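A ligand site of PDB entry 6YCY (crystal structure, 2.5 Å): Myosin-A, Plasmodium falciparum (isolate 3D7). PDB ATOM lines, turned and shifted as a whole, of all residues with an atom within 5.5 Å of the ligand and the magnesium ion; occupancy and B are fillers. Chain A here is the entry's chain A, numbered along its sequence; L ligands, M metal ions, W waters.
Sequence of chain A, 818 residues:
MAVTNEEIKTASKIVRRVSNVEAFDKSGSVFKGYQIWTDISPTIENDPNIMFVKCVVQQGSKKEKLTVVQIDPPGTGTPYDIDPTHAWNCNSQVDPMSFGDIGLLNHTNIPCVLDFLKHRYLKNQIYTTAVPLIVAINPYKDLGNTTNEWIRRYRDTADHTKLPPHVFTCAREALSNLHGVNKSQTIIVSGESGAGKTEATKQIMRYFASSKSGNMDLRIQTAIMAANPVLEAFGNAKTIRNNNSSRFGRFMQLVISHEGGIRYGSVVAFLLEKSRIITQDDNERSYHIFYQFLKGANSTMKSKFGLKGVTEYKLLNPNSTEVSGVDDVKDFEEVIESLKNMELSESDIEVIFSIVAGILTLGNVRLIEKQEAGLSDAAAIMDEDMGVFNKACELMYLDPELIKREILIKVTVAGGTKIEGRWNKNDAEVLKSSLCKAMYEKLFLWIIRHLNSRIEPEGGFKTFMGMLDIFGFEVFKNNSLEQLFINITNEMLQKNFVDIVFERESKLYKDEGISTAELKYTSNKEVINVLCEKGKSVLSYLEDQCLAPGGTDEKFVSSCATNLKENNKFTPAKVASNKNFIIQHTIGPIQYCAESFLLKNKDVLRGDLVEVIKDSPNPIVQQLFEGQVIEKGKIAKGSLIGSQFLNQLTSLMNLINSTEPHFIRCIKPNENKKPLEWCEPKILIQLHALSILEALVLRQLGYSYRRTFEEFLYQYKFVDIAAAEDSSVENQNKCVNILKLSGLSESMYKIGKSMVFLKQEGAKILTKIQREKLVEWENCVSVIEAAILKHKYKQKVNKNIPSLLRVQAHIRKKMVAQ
Water W1 lies within hydrogen-bond range of the side-chain carboxylate of Asp 469 (2.6 Å) and the side-chain amino group of Lys 197 (2.8 Å).
Water W2 lies within hydrogen-bond range of O of Asn 244 (2.7 Å), O4 of the ligand (2.7 Å) and OG of Ser 246 (3.1 Å).
Water W3 lies within hydrogen-bond range of O3 of the ligand (2.7 Å), OG of Ser 245 (3.1 Å) and N of Ser 246 (3.4 Å).
Water W4 lies within hydrogen-bond range of a nitrogen (N4) of the ligand, the backbone NH of Leu 143 and the side-chain carboxylate of Asp 142.
Residues that only touch the magnesium ion: Lys 197 (3.9 Å) and Asp 469 (3.99 Å).
Of the 25 residues printed, 4 come within 4 Å of the magnesium ion.
The nearest printed residue that does not touch the magnesium ion is Asn 244 (5.1 Å).
The magnesium ion is bound by OG1 of Thr 198 (1.9 Å), water W1 (2.3 Å), O1 of the ligand (2.3 Å) and water W2 (2.4 Å).
The magnesium ion has four donor atoms within binding distance.
Slightly farther from the magnesium ion lies the side-chain hydroxyl (OG) of Ser 246 (2.7 Å).
OH of Tyr 140 lies within hydrogen-bond range of O of Gly 194, 3.2 Å away.
N of Asn 244 lies close to OD1 of Asn 242 (3.2 Å).
OG1 of Thr 198 sits close to OD2 of Asp 469.
The side-chain hydroxyl of Ser 245 sits at hydrogen-bond distance from the side-chain hydroxyl of Ser 193, at 3.4 Å.
OD1 of Asn 244 sits at hydrogen-bond distance from ND2 of Asn 236.
OG1 of Thr 198 lies close to OG of Ser 246 (3.3 Å).
The side-chain amide oxygen (OD1) of Asn 236 is in hydrogen-bond range of the side-chain hydroxyl (OG) of Ser 246 (3.0 Å).
The backbone carbonyl oxygen (O) of Gly 194 is in hydrogen-bond range of the side-chain amide nitrogen (ND2) of Asn 138 (2.6 Å).
The backbone NH (N) of Gly 194 is in hydrogen-bond range of an oxygen (O3) of the ligand (2.8 Å).
The backbone NH (N) of Gly 196 lies within hydrogen-bond range of an oxygen (O6) of the ligand (3.0 Å).
The side-chain amino group (NZ) of Lys 197 is in salt-bridge range of an oxygen (O2) of the ligand, at 2.8 Å.
N3 of the ligand lies close to NE2 of Gln 203, 3.4 Å away.
ND2 of Asn 242 sits at hydrogen-bond distance from O3 of the ligand (2.7 Å).
An oxygen (O5) of the ligand lies within hydrogen-bond range of the backbone NH of Thr 198, at 3.0 Å.
The backbone NH (N) of Lys 197 lies close to an oxygen (O2) of the ligand (3.2 Å).
The side-chain amide nitrogen (ND2) of Asn 138 lies within hydrogen-bond range of an oxygen (O8) of the ligand (2.8 Å).
The backbone NH (N) of Ala 195 lies within hydrogen-bond range of an oxygen (O2) of the ligand, at 3.5 Å.
O5 of the ligand sits at hydrogen-bond distance from N of Glu 199, 2.9 Å away.
O of Glu 192 sits close to O2 of the ligand (3.2 Å).
O of Asn 244 lies close to O4 of the ligand, at 3.5 Å.
Residues that only touch the ligand: Lys 141 (3.1 Å), Tyr 140 (3.5 Å), Ser 193 (3.6 Å) and Pro 139 (3.6 Å).
Hydrophobic or aromatic side chains within 4 Å of the ligand: Pro 139, Tyr 140 and Ala 195.
Within 4 Å of the ligand: Asn 138, Pro 139, Tyr 140, Lys 141, Glu 192, Ser 193, Gly 194, Ala 195, Gly 196, Lys 197, Thr 198, Glu 199, Gln 203, Asn 242 and Asn 244.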
ATOM      1  N   ILE A 126     -10.157 -20.405  20.079  1.00  0.00           N
ATOM      2  CA  ILE A 126      -9.425 -19.269  19.549  1.00  0.00           C
ATOM      3  C   ILE A 126      -8.093 -19.026  20.249  1.00  0.00           C
ATOM      4  O   ILE A 126      -7.314 -18.222  19.758  1.00  0.00           O
ATOM      5  CB  ILE A 126     -10.332 -17.989  19.506  1.00  0.00           C
ATOM      6  CG1 ILE A 126     -10.778 -17.504  20.916  1.00  0.00           C
ATOM      7  CG2 ILE A 126     -11.563 -18.220  18.568  1.00  0.00           C
ATOM      8  CD1 ILE A 126     -10.852 -15.979  21.040  1.00  0.00           C
ATOM      9  N   TYR A 127      -7.793 -19.742  21.334  1.00  0.00           N
ATOM     10  CA  TYR A 127      -6.545 -19.582  22.078  1.00  0.00           C
ATOM     11  C   TYR A 127      -5.669 -20.820  21.957  1.00  0.00           C
ATOM     12  O   TYR A 127      -6.153 -21.950  22.122  1.00  0.00           O
ATOM     13  CB  TYR A 127      -6.738 -19.171  23.570  1.00  0.00           C
ATOM     14  CG  TYR A 127      -7.781 -18.103  23.830  1.00  0.00           C
ATOM     15  CD1 TYR A 127      -7.511 -16.765  23.595  1.00  0.00           C
ATOM     16  CD2 TYR A 127      -9.031 -18.429  24.350  1.00  0.00           C
ATOM     17  CE1 TYR A 127      -8.482 -15.787  23.813  1.00  0.00           C
ATOM     18  CE2 TYR A 127      -9.974 -17.455  24.643  1.00  0.00           C
ATOM     19  CZ  TYR A 127      -9.701 -16.134  24.365  1.00  0.00           C
ATOM     20  OH  TYR A 127     -10.681 -15.185  24.572  1.00  0.00           O
ATOM     21  N   ASN A 138      -9.361 -13.594  16.548  1.00  0.00           N
ATOM     22  CA  ASN A 138     -10.683 -12.953  16.679  1.00  0.00           C
ATOM     23  C   ASN A 138     -11.865 -13.809  16.107  1.00  0.00           C
ATOM     24  O   ASN A 138     -11.954 -14.019  14.889  1.00  0.00           O
ATOM     25  CB  ASN A 138     -10.646 -11.544  16.080  1.00  0.00           C
ATOM     26  CG  ASN A 138     -11.809 -10.644  16.408  1.00  0.00           C
ATOM     27  OD1 ASN A 138     -12.888 -11.059  16.861  1.00  0.00           O
ATOM     28  ND2 ASN A 138     -11.655  -9.398  16.069  1.00  0.00           N
ATOM     29  N   PRO A 139     -12.809 -14.277  16.958  1.00  0.00           N
ATOM     30  CA  PRO A 139     -13.932 -15.050  16.420  1.00  0.00           C
ATOM     31  C   PRO A 139     -15.018 -14.204  15.760  1.00  0.00           C
ATOM     32  O   PRO A 139     -15.920 -14.778  15.154  1.00  0.00           O
ATOM     33  CB  PRO A 139     -14.463 -15.768  17.662  1.00  0.00           C
ATOM     34  CG  PRO A 139     -14.201 -14.826  18.779  1.00  0.00           C
ATOM     35  CD  PRO A 139     -12.918 -14.109  18.423  1.00  0.00           C
ATOM     36  N   TYR A 140     -14.968 -12.850  15.894  1.00  0.00           N
ATOM     37  CA  TYR A 140     -15.955 -11.896  15.364  1.00  0.00           C
ATOM     38  C   TYR A 140     -17.397 -12.292  15.675  1.00  0.00           C
ATOM     39  O   TYR A 140     -18.292 -12.108  14.843  1.00  0.00           O
ATOM     40  CB  TYR A 140     -15.747 -11.630  13.875  1.00  0.00           C
ATOM     41  CG  TYR A 140     -14.685 -10.595  13.571  1.00  0.00           C
ATOM     42  CD1 TYR A 140     -14.842  -9.264  13.967  1.00  0.00           C
ATOM     43  CD2 TYR A 140     -13.544 -10.924  12.826  1.00  0.00           C
ATOM     44  CE1 TYR A 140     -13.886  -8.299  13.662  1.00  0.00           C
ATOM     45  CE2 TYR A 140     -12.592  -9.958  12.501  1.00  0.00           C
ATOM     46  CZ  TYR A 140     -12.758  -8.652  12.939  1.00  0.00           C
ATOM     47  OH  TYR A 140     -11.834  -7.680  12.632  1.00  0.00           O
ATOM     48  N   LYS A 141     -17.602 -12.865  16.884  1.00  0.00           N
ATOM     49  CA  LYS A 141     -18.864 -13.319  17.469  1.00  0.00           C
ATOM     50  C   LYS A 141     -18.659 -13.626  18.943  1.00  0.00           C
ATOM     51  O   LYS A 141     -17.532 -13.913  19.376  1.00  0.00           O
ATOM     52  CB  LYS A 141     -19.507 -14.509  16.690  1.00  0.00           C
ATOM     53  CG  LYS A 141     -18.989 -15.911  17.008  1.00  0.00           C
ATOM     54  CD  LYS A 141     -19.717 -16.964  16.196  1.00  0.00           C
ATOM     55  CE  LYS A 141     -19.037 -18.332  16.192  1.00  0.00           C
ATOM     56  NZ  LYS A 141     -17.711 -18.338  15.520  1.00  0.00           N
ATOM     57  N   ASP A 142     -19.739 -13.548  19.740  1.00  0.00           N
ATOM     58  CA  ASP A 142     -19.641 -13.849  21.156  1.00  0.00           C
ATOM     59  C   ASP A 142     -19.680 -15.360  21.317  1.00  0.00           C
ATOM     60  O   ASP A 142     -20.695 -16.002  21.009  1.00  0.00           O
ATOM     61  CB  ASP A 142     -20.738 -13.139  21.970  1.00  0.00           C
ATOM     62  CG  ASP A 142     -20.663 -13.291  23.494  1.00  0.00           C
ATOM     63  OD1 ASP A 142     -19.535 -13.357  24.045  1.00  0.00           O
ATOM     64  OD2 ASP A 142     -21.740 -13.279  24.131  1.00  0.00           O
ATOM     65  N   LEU A 143     -18.541 -15.938  21.746  1.00  0.00           N
ATOM     66  CA  LEU A 143     -18.422 -17.369  21.969  1.00  0.00           C
ATOM     67  C   LEU A 143     -18.958 -17.725  23.331  1.00  0.00           C
ATOM     68  O   LEU A 143     -19.173 -18.901  23.616  1.00  0.00           O
ATOM     69  CB  LEU A 143     -16.949 -17.837  21.868  1.00  0.00           C
ATOM     70  CG  LEU A 143     -16.152 -17.515  20.598  1.00  0.00           C
ATOM     71  CD1 LEU A 143     -14.707 -17.939  20.764  1.00  0.00           C
ATOM     72  CD2 LEU A 143     -16.800 -18.095  19.318  1.00  0.00           C
ATOM     73  N   GLY A 191      -1.073  -6.811  18.494  1.00  0.00           N
ATOM     74  CA  GLY A 191      -1.736  -7.245  17.268  1.00  0.00           C
ATOM     75  C   GLY A 191      -2.102  -6.080  16.395  1.00  0.00           C
ATOM     76  O   GLY A 191      -1.794  -4.944  16.743  1.00  0.00           O
ATOM     77  N   GLU A 192      -2.717  -6.346  15.242  1.00  0.00           N
ATOM     78  CA  GLU A 192      -3.123  -5.291  14.318  1.00  0.00           C
ATOM     79  C   GLU A 192      -4.543  -4.797  14.625  1.00  0.00           C
ATOM     80  O   GLU A 192      -5.223  -5.399  15.437  1.00  0.00           O
ATOM     81  CB  GLU A 192      -2.952  -5.736  12.850  1.00  0.00           C
ATOM     82  CG  GLU A 192      -3.932  -6.771  12.354  1.00  0.00           C
ATOM     83  CD  GLU A 192      -3.736  -7.154  10.894  1.00  0.00           C
ATOM     84  OE1 GLU A 192      -2.584  -7.154  10.416  1.00  0.00           O
ATOM     85  OE2 GLU A 192      -4.745  -7.503  10.247  1.00  0.00           O
ATOM     86  N   SER A 193      -4.984  -3.710  13.979  1.00  0.00           N
ATOM     87  CA  SER A 193      -6.307  -3.149  14.206  1.00  0.00           C
ATOM     88  C   SER A 193      -7.373  -4.164  13.844  1.00  0.00           C
ATOM     89  O   SER A 193      -7.407  -4.628  12.699  1.00  0.00           O
ATOM     90  CB  SER A 193      -6.499  -1.872  13.383  1.00  0.00           C
ATOM     91  OG  SER A 193      -7.745  -1.271  13.699  1.00  0.00           O
ATOM     92  N   GLY A 194      -8.198  -4.513  14.830  1.00  0.00           N
ATOM     93  CA  GLY A 194      -9.319  -5.433  14.693  1.00  0.00           C
ATOM     94  C   GLY A 194      -9.014  -6.820  15.174  1.00  0.00           C
ATOM     95  O   GLY A 194      -9.891  -7.686  15.139  1.00  0.00           O
ATOM     96  N   ALA A 195      -7.758  -7.058  15.652  1.00  0.00           N
ATOM     97  CA  ALA A 195      -7.257  -8.356  16.136  1.00  0.00           C
ATOM     98  C   ALA A 195      -7.926  -8.849  17.426  1.00  0.00           C
ATOM     99  O   ALA A 195      -7.909 -10.051  17.678  1.00  0.00           O
ATOM    100  CB  ALA A 195      -5.749  -8.302  16.321  1.00  0.00           C
ATOM    101  N   GLY A 196      -8.460  -7.935  18.239  1.00  0.00           N
ATOM    102  CA  GLY A 196      -9.131  -8.294  19.498  1.00  0.00           C
ATOM    103  C   GLY A 196      -8.404  -7.940  20.785  1.00  0.00           C
ATOM    104  O   GLY A 196      -8.715  -8.499  21.845  1.00  0.00           O
ATOM    105  N   LYS A 197      -7.410  -7.000  20.686  1.00  0.00           N
ATOM    106  CA  LYS A 197      -6.553  -6.506  21.790  1.00  0.00           C
ATOM    107  C   LYS A 197      -7.319  -5.863  22.904  1.00  0.00           C
ATOM    108  O   LYS A 197      -7.034  -6.153  24.052  1.00  0.00           O
ATOM    109  CB  LYS A 197      -5.562  -5.472  21.307  1.00  0.00           C
ATOM    110  CG  LYS A 197      -4.521  -5.910  20.330  1.00  0.00           C
ATOM    111  CD  LYS A 197      -3.512  -4.767  20.221  1.00  0.00           C
ATOM    112  CE  LYS A 197      -3.654  -3.997  18.940  1.00  0.00           C
ATOM    113  NZ  LYS A 197      -4.814  -3.105  18.907  1.00  0.00           N
ATOM    114  N   THR A 198      -8.249  -4.942  22.573  1.00  0.00           N
ATOM    115  CA  THR A 198      -9.053  -4.209  23.558  1.00  0.00           C
ATOM    116  C   THR A 198      -9.998  -5.177  24.241  1.00  0.00           C
ATOM    117  O   THR A 198     -10.138  -5.120  25.459  1.00  0.00           O
ATOM    118  CB  THR A 198      -9.701  -2.960  22.899  1.00  0.00           C
ATOM    119  OG1 THR A 198      -8.651  -2.094  22.453  1.00  0.00           O
ATOM    120  CG2 THR A 198     -10.602  -2.192  23.836  1.00  0.00           C
ATOM    121  N   GLU A 199     -10.561  -6.139  23.479  1.00  0.00           N
ATOM    122  CA  GLU A 199     -11.405  -7.170  24.073  1.00  0.00           C
ATOM    123  C   GLU A 199     -10.650  -8.054  25.032  1.00  0.00           C
ATOM    124  O   GLU A 199     -11.097  -8.189  26.162  1.00  0.00           O
ATOM    125  CB  GLU A 199     -12.176  -7.986  23.050  1.00  0.00           C
ATOM    126  CG  GLU A 199     -13.285  -7.184  22.403  1.00  0.00           C
ATOM    127  CD  GLU A 199     -14.254  -6.505  23.360  1.00  0.00           C
ATOM    128  OE1 GLU A 199     -14.826  -7.194  24.244  1.00  0.00           O
ATOM    129  OE2 GLU A 199     -14.410  -5.269  23.246  1.00  0.00           O
ATOM    130  N   ALA A 200      -9.465  -8.552  24.634  1.00  0.00           N
ATOM    131  CA  ALA A 200      -8.621  -9.380  25.515  1.00  0.00           C
ATOM    132  C   ALA A 200      -8.260  -8.635  26.790  1.00  0.00           C
ATOM    133  O   ALA A 200      -8.286  -9.249  27.853  1.00  0.00           O
ATOM    134  CB  ALA A 200      -7.353  -9.799  24.785  1.00  0.00           C
ATOM    135  N   GLN A 203     -11.389  -8.307  29.037  1.00  0.00           N
ATOM    136  CA  GLN A 203     -11.612  -9.657  29.570  1.00  0.00           C
ATOM    137  C   GLN A 203     -10.689  -9.951  30.757  1.00  0.00           C
ATOM    138  O   GLN A 203     -11.157 -10.481  31.773  1.00  0.00           O
ATOM    139  CB  GLN A 203     -11.379 -10.717  28.487  1.00  0.00           C
ATOM    140  CG  GLN A 203     -12.544 -10.859  27.519  1.00  0.00           C
ATOM    141  CD  GLN A 203     -12.211 -11.378  26.142  1.00  0.00           C
ATOM    142  OE1 GLN A 203     -11.115 -11.893  25.846  1.00  0.00           O
ATOM    143  NE2 GLN A 203     -13.199 -11.299  25.252  1.00  0.00           N
ATOM    144  N   ASN A 236     -11.146   6.081  20.919  1.00  0.00           N
ATOM    145  CA  ASN A 236     -11.444   5.078  19.889  1.00  0.00           C
ATOM    146  C   ASN A 236     -12.374   5.673  18.827  1.00  0.00           C
ATOM    147  O   ASN A 236     -13.222   6.502  19.150  1.00  0.00           O
ATOM    148  CB  ASN A 236     -12.114   3.824  20.458  1.00  0.00           C
ATOM    149  CG  ASN A 236     -11.298   2.896  21.297  1.00  0.00           C
ATOM    150  OD1 ASN A 236     -10.329   3.279  21.966  1.00  0.00           O
ATOM    151  ND2 ASN A 236     -11.771   1.675  21.371  1.00  0.00           N
ATOM    152  N   ASN A 242     -11.847  -1.363  11.585  1.00  0.00           N
ATOM    153  CA  ASN A 242     -12.358  -1.556  12.952  1.00  0.00           C
ATOM    154  C   ASN A 242     -13.359  -0.467  13.369  1.00  0.00           C
ATOM    155  O   ASN A 242     -13.006   0.706  13.474  1.00  0.00           O
ATOM    156  CB  ASN A 242     -11.180  -1.566  13.947  1.00  0.00           C
ATOM    157  CG  ASN A 242     -11.442  -2.081  15.349  1.00  0.00           C
ATOM    158  OD1 ASN A 242     -12.546  -2.493  15.736  1.00  0.00           O
ATOM    159  ND2 ASN A 242     -10.386  -2.073  16.126  1.00  0.00           N
ATOM    160  N   ASN A 244     -14.431   0.042  16.302  1.00  0.00           N
ATOM    161  CA  ASN A 244     -14.022   0.535  17.620  1.00  0.00           C
ATOM    162  C   ASN A 244     -12.482   0.466  17.748  1.00  0.00           C
ATOM    163  O   ASN A 244     -11.946  -0.227  18.605  1.00  0.00           O
ATOM    164  CB  ASN A 244     -14.760  -0.222  18.743  1.00  0.00           C
ATOM    165  CG  ASN A 244     -14.582   0.354  20.131  1.00  0.00           C
ATOM    166  OD1 ASN A 244     -14.348   1.550  20.315  1.00  0.00           O
ATOM    167  ND2 ASN A 244     -14.667  -0.482  21.140  1.00  0.00           N
ATOM    168  N   SER A 245     -11.791   1.206  16.871  1.00  0.00           N
ATOM    169  CA  SER A 245     -10.333   1.233  16.859  1.00  0.00           C
ATOM    170  C   SER A 245      -9.757   2.151  17.892  1.00  0.00           C
ATOM    171  O   SER A 245     -10.080   3.342  17.884  1.00  0.00           O
ATOM    172  CB  SER A 245      -9.804   1.610  15.480  1.00  0.00           C
ATOM    173  OG  SER A 245      -8.381   1.564  15.461  1.00  0.00           O
ATOM    174  N   SER A 246      -8.842   1.626  18.736  1.00  0.00           N
ATOM    175  CA  SER A 246      -8.062   2.375  19.721  1.00  0.00           C
ATOM    176  C   SER A 246      -7.003   3.171  18.949  1.00  0.00           C
ATOM    177  O   SER A 246      -6.218   2.597  18.196  1.00  0.00           O
ATOM    178  CB  SER A 246      -7.415   1.427  20.720  1.00  0.00           C
ATOM    179  OG  SER A 246      -8.338   1.077  21.729  1.00  0.00           O
ATOM    180  N   ASP A 469      -1.535  -2.403  25.980  1.00  0.00           N
ATOM    181  CA  ASP A 469      -2.493  -2.677  24.904  1.00  0.00           C
ATOM    182  C   ASP A 469      -2.050  -1.777  23.777  1.00  0.00           C
ATOM    183  O   ASP A 469      -2.356  -0.583  23.755  1.00  0.00           O
ATOM    184  CB  ASP A 469      -3.936  -2.425  25.405  1.00  0.00           C
ATOM    185  CG  ASP A 469      -5.035  -2.555  24.372  1.00  0.00           C
ATOM    186  OD1 ASP A 469      -4.730  -2.968  23.246  1.00  0.00           O
ATOM    187  OD2 ASP A 469      -6.192  -2.198  24.681  1.00  0.00           O
HETATM  188  P1  LIG L   1      -7.977  -4.043  18.421  1.00  0.00           P
HETATM  189  O1  LIG L   1      -7.925  -3.245  19.678  1.00  0.00           O
HETATM  190  O2  LIG L   1      -6.747  -4.970  18.240  1.00  0.00           O
HETATM  191  O3  LIG L   1      -8.141  -3.155  17.246  1.00  0.00           O
HETATM  192  P2  LIG L   1     -10.590  -4.915  19.203  1.00  0.00           P
HETATM  193  O4  LIG L   1     -10.938  -3.470  19.259  1.00  0.00           O
HETATM  194  O5  LIG L   1     -10.534  -5.515  20.649  1.00  0.00           O
HETATM  195  O6  LIG L   1      -9.195  -5.048  18.454  1.00  0.00           O
HETATM  196  O7  LIG L   1     -11.481  -5.861  18.270  1.00  0.00           O
HETATM  197  C1  LIG L   1     -12.212  -5.391  17.113  1.00  0.00           C
HETATM  198  C2  LIG L   1     -13.577  -6.025  17.133  1.00  0.00           C
HETATM  199  O8  LIG L   1     -13.451  -7.455  17.015  1.00  0.00           O
HETATM  200  C3  LIG L   1     -14.381  -5.814  18.411  1.00  0.00           C
HETATM  201  O9  LIG L   1     -14.940  -4.499  18.568  1.00  0.00           O
HETATM  202  C4  LIG L   1     -15.343  -7.011  18.382  1.00  0.00           C
HETATM  203  O10 LIG L   1     -16.448  -6.883  17.501  1.00  0.00           O
HETATM  204  C5  LIG L   1     -14.423  -8.104  17.828  1.00  0.00           C
HETATM  205  N1  LIG L   1     -13.765  -8.913  18.856  1.00  0.00           N
HETATM  206  C6  LIG L   1     -12.483  -8.774  19.324  1.00  0.00           C
HETATM  207  N2  LIG L   1     -12.126  -9.678  20.197  1.00  0.00           N
HETATM  208  C7  LIG L   1     -13.264 -10.472  20.329  1.00  0.00           C
HETATM  209  C8  LIG L   1     -13.557 -11.592  21.130  1.00  0.00           C
HETATM  210  N3  LIG L   1     -12.671 -12.150  21.968  1.00  0.00           N
HETATM  211  N4  LIG L   1     -14.792 -12.133  21.044  1.00  0.00           N
HETATM  212  C9  LIG L   1     -15.679 -11.575  20.206  1.00  0.00           C
HETATM  213  N5  LIG L   1     -15.523 -10.519  19.401  1.00  0.00           N
HETATM  214  C10 LIG L   1     -14.280  -9.999  19.514  1.00  0.00           C
HETATM  215 MG    MG M   1      -7.605  -1.416  20.956  1.00  0.00          MG
HETATM  216  O   HOH W   1      -5.366  -1.535  21.147  1.00  0.00           O
HETATM  217  O   HOH W   2      -9.815  -1.094  20.022  1.00  0.00           O
HETATM  218  O   HOH W   3      -6.996  -0.692  17.074  1.00  0.00           O
HETATM  219  O   HOH W   4     -16.452 -13.861  22.906  1.00  0.00           O
HETATM  220  O   HOH W   5     -15.075  -4.421  14.482  1.00  0.00           O
